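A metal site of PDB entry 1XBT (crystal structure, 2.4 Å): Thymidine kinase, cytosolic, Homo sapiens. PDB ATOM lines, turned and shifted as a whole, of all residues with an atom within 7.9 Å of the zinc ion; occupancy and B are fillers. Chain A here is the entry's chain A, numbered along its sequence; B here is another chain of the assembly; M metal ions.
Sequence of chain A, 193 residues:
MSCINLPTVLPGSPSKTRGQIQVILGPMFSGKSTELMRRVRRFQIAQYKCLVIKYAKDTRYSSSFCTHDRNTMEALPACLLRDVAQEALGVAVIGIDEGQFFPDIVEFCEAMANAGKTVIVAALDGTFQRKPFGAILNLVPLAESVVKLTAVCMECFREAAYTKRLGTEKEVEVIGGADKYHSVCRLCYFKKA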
ATOM      1  N   VAL A 152      13.128 -11.343  -3.273  1.00  0.00           N
ATOM      2  CA  VAL A 152      14.272 -10.450  -3.305  1.00  0.00           C
ATOM      3  C   VAL A 152      14.867 -10.463  -4.719  1.00  0.00           C
ATOM      4  O   VAL A 152      15.055 -11.528  -5.303  1.00  0.00           O
ATOM      5  CB  VAL A 152      15.303 -10.846  -2.232  1.00  0.00           C
ATOM      6  CG1 VAL A 152      16.601 -10.036  -2.373  1.00  0.00           C
ATOM      7  CG2 VAL A 152      14.695 -10.661  -0.827  1.00  0.00           C
ATOM      8  N   CYS A 153      15.130  -9.275  -5.274  1.00  0.00           N
ATOM      9  CA  CYS A 153      15.761  -9.153  -6.591  1.00  0.00           C
ATOM     10  C   CYS A 153      17.133  -9.782  -6.564  1.00  0.00           C
ATOM     11  O   CYS A 153      17.987  -9.362  -5.807  1.00  0.00           O
ATOM     12  CB  CYS A 153      15.868  -7.683  -7.034  1.00  0.00           C
ATOM     13  SG  CYS A 153      16.474  -7.428  -8.729  1.00  0.00           S
ATOM     14  N   MET A 154      17.327 -10.801  -7.390  1.00  0.00           N
ATOM     15  CA  MET A 154      18.591 -11.527  -7.437  1.00  0.00           C
ATOM     16  C   MET A 154      19.686 -10.752  -8.171  1.00  0.00           C
ATOM     17  O   MET A 154      20.835 -11.204  -8.241  1.00  0.00           O
ATOM     18  CB  MET A 154      18.376 -12.901  -8.081  1.00  0.00           C
ATOM     19  CG  MET A 154      17.704 -13.898  -7.164  1.00  0.00           C
ATOM     20  SD  MET A 154      17.018 -15.266  -8.078  1.00  0.00           S
ATOM     21  CE  MET A 154      16.524 -16.399  -6.758  1.00  0.00           C
ATOM     22  N   GLU A 155      19.351  -9.579  -8.686  1.00  0.00           N
ATOM     23  CA  GLU A 155      20.318  -8.777  -9.431  1.00  0.00           C
ATOM     24  C   GLU A 155      20.711  -7.470  -8.731  1.00  0.00           C
ATOM     25  O   GLU A 155      21.854  -7.039  -8.832  1.00  0.00           O
ATOM     26  CB  GLU A 155      19.838  -8.548 -10.873  1.00  0.00           C
ATOM     27  CG  GLU A 155      20.092  -9.743 -11.772  1.00  0.00           C
ATOM     28  CD  GLU A 155      19.124  -9.877 -12.939  1.00  0.00           C
ATOM     29  OE1 GLU A 155      18.752 -11.033 -13.258  1.00  0.00           O
ATOM     30  OE2 GLU A 155      18.761  -8.860 -13.571  1.00  0.00           O
ATOM     31  N   CYS A 156      19.766  -6.855  -8.012  1.00  0.00           N
ATOM     32  CA  CYS A 156      20.044  -5.613  -7.283  1.00  0.00           C
ATOM     33  C   CYS A 156      19.672  -5.690  -5.807  1.00  0.00           C
ATOM     34  O   CYS A 156      19.945  -4.752  -5.049  1.00  0.00           O
ATOM     35  CB  CYS A 156      19.397  -4.395  -7.966  1.00  0.00           C
ATOM     36  SG  CYS A 156      17.690  -3.990  -7.473  1.00  0.00           S
ATOM     37  N   PHE A 157      19.044  -6.789  -5.406  1.00  0.00           N
ATOM     38  CA  PHE A 157      18.725  -7.083  -3.998  1.00  0.00           C
ATOM     39  C   PHE A 157      17.674  -6.191  -3.331  1.00  0.00           C
ATOM     40  O   PHE A 157      17.531  -6.202  -2.099  1.00  0.00           O
ATOM     41  CB  PHE A 157      20.008  -7.201  -3.151  1.00  0.00           C
ATOM     42  CG  PHE A 157      21.106  -7.956  -3.853  1.00  0.00           C
ATOM     43  CD1 PHE A 157      22.216  -7.284  -4.346  1.00  0.00           C
ATOM     44  CD2 PHE A 157      21.007  -9.327  -4.052  1.00  0.00           C
ATOM     45  CE1 PHE A 157      23.234  -7.979  -5.006  1.00  0.00           C
ATOM     46  CE2 PHE A 157      21.998 -10.035  -4.713  1.00  0.00           C
ATOM     47  CZ  PHE A 157      23.128  -9.360  -5.192  1.00  0.00           C
ATOM     48  N   ARG A 158      16.931  -5.436  -4.126  1.00  0.00           N
ATOM     49  CA  ARG A 158      15.728  -4.753  -3.653  1.00  0.00           C
ATOM     50  C   ARG A 158      14.526  -5.711  -3.744  1.00  0.00           C
ATOM     51  O   ARG A 158      14.690  -6.893  -4.048  1.00  0.00           O
ATOM     52  CB  ARG A 158      15.512  -3.457  -4.448  1.00  0.00           C
ATOM     53  CG  ARG A 158      16.536  -2.381  -4.114  1.00  0.00           C
ATOM     54  CD  ARG A 158      16.403  -1.088  -4.905  1.00  0.00           C
ATOM     55  NE  ARG A 158      16.016   0.035  -4.050  1.00  0.00           N
ATOM     56  CZ  ARG A 158      16.296   1.319  -4.292  1.00  0.00           C
ATOM     57  NH1 ARG A 158      16.982   1.664  -5.388  1.00  0.00           N
ATOM     58  NH2 ARG A 158      15.882   2.264  -3.457  1.00  0.00           N
ATOM     59  N   GLU A 159      13.332  -5.208  -3.456  1.00  0.00           N
ATOM     60  CA  GLU A 159      12.128  -6.043  -3.516  1.00  0.00           C
ATOM     61  C   GLU A 159      11.792  -6.429  -4.953  1.00  0.00           C
ATOM     62  O   GLU A 159      11.821  -5.597  -5.857  1.00  0.00           O
ATOM     63  CB  GLU A 159      10.943  -5.328  -2.895  1.00  0.00           C
ATOM     64  CG  GLU A 159      10.902  -5.419  -1.380  1.00  0.00           C
ATOM     65  CD  GLU A 159       9.499  -5.211  -0.823  1.00  0.00           C
ATOM     66  OE1 GLU A 159       8.728  -4.399  -1.397  1.00  0.00           O
ATOM     67  OE2 GLU A 159       9.178  -5.860   0.213  1.00  0.00           O
ATOM     68  N   ALA A 160      11.462  -7.713  -5.165  1.00  0.00           N
ATOM     69  CA  ALA A 160      11.167  -8.249  -6.487  1.00  0.00           C
ATOM     70  C   ALA A 160       9.701  -8.649  -6.608  1.00  0.00           C
ATOM     71  O   ALA A 160       9.166  -9.365  -5.746  1.00  0.00           O
ATOM     72  CB  ALA A 160      12.059  -9.439  -6.774  1.00  0.00           C
ATOM     73  N   SER A 183      14.184 -13.978  -9.713  1.00  0.00           N
ATOM     74  CA  SER A 183      13.213 -12.995  -9.233  1.00  0.00           C
ATOM     75  C   SER A 183      13.851 -11.633  -9.381  1.00  0.00           C
ATOM     76  O   SER A 183      15.023 -11.440  -9.099  1.00  0.00           O
ATOM     77  CB  SER A 183      12.822 -13.252  -7.781  1.00  0.00           C
ATOM     78  OG  SER A 183      13.949 -13.265  -6.923  1.00  0.00           O
ATOM     79  N   VAL A 184      13.054 -10.663  -9.812  1.00  0.00           N
ATOM     80  CA  VAL A 184      13.616  -9.413 -10.269  1.00  0.00           C
ATOM     81  C   VAL A 184      12.668  -8.220 -10.046  1.00  0.00           C
ATOM     82  O   VAL A 184      11.444  -8.377 -10.055  1.00  0.00           O
ATOM     83  CB  VAL A 184      14.030  -9.617 -11.767  1.00  0.00           C
ATOM     84  CG1 VAL A 184      13.219  -8.795 -12.717  1.00  0.00           C
ATOM     85  CG2 VAL A 184      15.533  -9.486 -11.958  1.00  0.00           C
ATOM     86  N   CYS A 185      13.227  -7.036  -9.800  1.00  0.00           N
ATOM     87  CA  CYS A 185      12.417  -5.815  -9.717  1.00  0.00           C
ATOM     88  C   CYS A 185      12.114  -5.284 -11.126  1.00  0.00           C
ATOM     89  O   CYS A 185      12.576  -5.839 -12.117  1.00  0.00           O
ATOM     90  CB  CYS A 185      13.135  -4.737  -8.902  1.00  0.00           C
ATOM     91  SG  CYS A 185      14.592  -4.080  -9.775  1.00  0.00           S
ATOM     92  N   ARG A 186      11.359  -4.187 -11.192  1.00  0.00           N
ATOM     93  CA  ARG A 186      11.006  -3.583 -12.467  1.00  0.00           C
ATOM     94  C   ARG A 186      12.227  -3.177 -13.308  1.00  0.00           C
ATOM     95  O   ARG A 186      12.298  -3.496 -14.495  1.00  0.00           O
ATOM     96  CB  ARG A 186      10.080  -2.375 -12.251  1.00  0.00           C
ATOM     97  CG  ARG A 186       9.619  -1.709 -13.537  1.00  0.00           C
ATOM     98  CD  ARG A 186       8.699  -0.515 -13.305  1.00  0.00           C
ATOM     99  NE  ARG A 186       7.425  -0.949 -12.741  1.00  0.00           N
ATOM    100  CZ  ARG A 186       6.381  -1.340 -13.455  1.00  0.00           C
ATOM    101  NH1 ARG A 186       6.447  -1.329 -14.785  1.00  0.00           N
ATOM    102  NH2 ARG A 186       5.263  -1.719 -12.840  1.00  0.00           N
ATOM    103  N   LEU A 187      13.171  -2.486 -12.688  1.00  0.00           N
ATOM    104  CA  LEU A 187      14.358  -1.983 -13.375  1.00  0.00           C
ATOM    105  C   LEU A 187      15.228  -3.108 -13.920  1.00  0.00           C
ATOM    106  O   LEU A 187      15.661  -3.062 -15.079  1.00  0.00           O
ATOM    107  CB  LEU A 187      15.166  -1.045 -12.467  1.00  0.00           C
ATOM    108  CG  LEU A 187      14.501   0.277 -12.054  1.00  0.00           C
ATOM    109  CD1 LEU A 187      15.507   1.243 -11.431  1.00  0.00           C
ATOM    110  CD2 LEU A 187      13.763   0.955 -13.214  1.00  0.00           C
ATOM    111  N   CYS A 188      15.476  -4.124 -13.094  1.00  0.00           N
ATOM    112  CA  CYS A 188      16.305  -5.242 -13.503  1.00  0.00           C
ATOM    113  C   CYS A 188      15.624  -6.128 -14.540  1.00  0.00           C
ATOM    114  O   CYS A 188      16.293  -6.737 -15.384  1.00  0.00           O
ATOM    115  CB  CYS A 188      16.783  -6.021 -12.287  1.00  0.00           C
ATOM    116  SG  CYS A 188      17.860  -5.018 -11.233  1.00  0.00           S
ATOM    117  N   TYR A 189      14.286  -6.185 -14.502  1.00  0.00           N
ATOM    118  CA  TYR A 189      13.516  -6.892 -15.520  1.00  0.00           C
ATOM    119  C   TYR A 189      13.817  -6.394 -16.936  1.00  0.00           C
ATOM    120  O   TYR A 189      13.930  -7.190 -17.873  1.00  0.00           O
ATOM    121  CB  TYR A 189      11.995  -6.792 -15.285  1.00  0.00           C
ATOM    122  CG  TYR A 189      11.205  -7.644 -16.260  1.00  0.00           C
ATOM    123  CD1 TYR A 189      11.019  -9.007 -16.026  1.00  0.00           C
ATOM    124  CD2 TYR A 189      10.668  -7.095 -17.424  1.00  0.00           C
ATOM    125  CE1 TYR A 189      10.322  -9.800 -16.917  1.00  0.00           C
ATOM    126  CE2 TYR A 189       9.967  -7.886 -18.325  1.00  0.00           C
ATOM    127  CZ  TYR A 189       9.795  -9.234 -18.071  1.00  0.00           C
ATOM    128  OH  TYR A 189       9.085 -10.025 -18.945  1.00  0.00           O
ATOM    129  N   LYS A 191      16.510  -4.541 -17.880  1.00  0.00           N
ATOM    130  CA  LYS A 191      17.934  -4.270 -18.102  1.00  0.00           C
ATOM    131  C   LYS A 191      18.527  -5.072 -19.264  1.00  0.00           C
ATOM    132  O   LYS A 191      18.358  -6.292 -19.333  1.00  0.00           O
ATOM    133  CB  LYS A 191      18.744  -4.532 -16.829  1.00  0.00           C
ATOM    134  CG  LYS A 191      18.911  -3.305 -15.958  1.00  0.00           C
ATOM    135  CD  LYS A 191      20.124  -3.432 -15.045  1.00  0.00           C
ATOM    136  CE  LYS A 191      20.601  -2.047 -14.606  1.00  0.00           C
ATOM    137  NZ  LYS A 191      21.815  -2.099 -13.720  1.00  0.00           N
ATOM    138  N   ARG B  18      12.338   5.402 -10.082  1.00  0.00           N
ATOM    139  CA  ARG B  18      11.819   4.151  -9.440  1.00  0.00           C
ATOM    140  C   ARG B  18      10.269   4.103  -9.410  1.00  0.00           C
ATOM    141  O   ARG B  18       9.645   4.355  -8.380  1.00  0.00           O
ATOM    142  CB  ARG B  18      12.392   4.024  -8.018  1.00  0.00           C
ATOM    143  CG  ARG B  18      12.528   2.604  -7.511  1.00  0.00           C
ATOM    144  CD  ARG B  18      13.920   1.997  -7.648  1.00  0.00           C
ATOM    145  NE  ARG B  18      13.835   0.539  -7.658  1.00  0.00           N
ATOM    146  CZ  ARG B  18      14.826  -0.287  -7.995  1.00  0.00           C
ATOM    147  NH1 ARG B  18      16.009   0.182  -8.357  1.00  0.00           N
ATOM    148  NH2 ARG B  18      14.602  -1.597  -7.957  1.00  0.00           N
HETATM  149 ZN    ZN M   1      16.567  -5.190  -9.192  1.00  0.00          ZN
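N of Glu 155 sits close to SG of Cys 153, at 3.6 Å.
The backbone NH of Cys 153 is in hydrogen-bond range of the backbone carbonyl oxygen of Arg 158, at 2.7 Å.
The side-chain sulfur (SG) of Cys 185 lies close to the guanidinium group (NH2) of Arg 18 of chain B, at 3.1 Å.
The side-chain sulfur of Cys 185 sits close to the backbone NH of Leu 187, at 3.6 Å.
The side-chain sulfur of Cys 156 lies close to the backbone NH of Arg 158 (3.7 Å).
Four residues have an atom within 4 Å of the zinc ion: Cys 153, Cys 156, Cys 185 and Cys 188.
The zinc ion is bound by the side-chain sulfur (SG) of Cys 153 (2.3 Å), the side-chain sulfur (SG) of Cys 185 (2.3 Å), the side-chain sulfur (SG) of Cys 156 (2.4 Å) and the side-chain sulfur (SG) of Cys 188 (2.4 Å).
The zinc ion has four donor atoms within binding distance.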
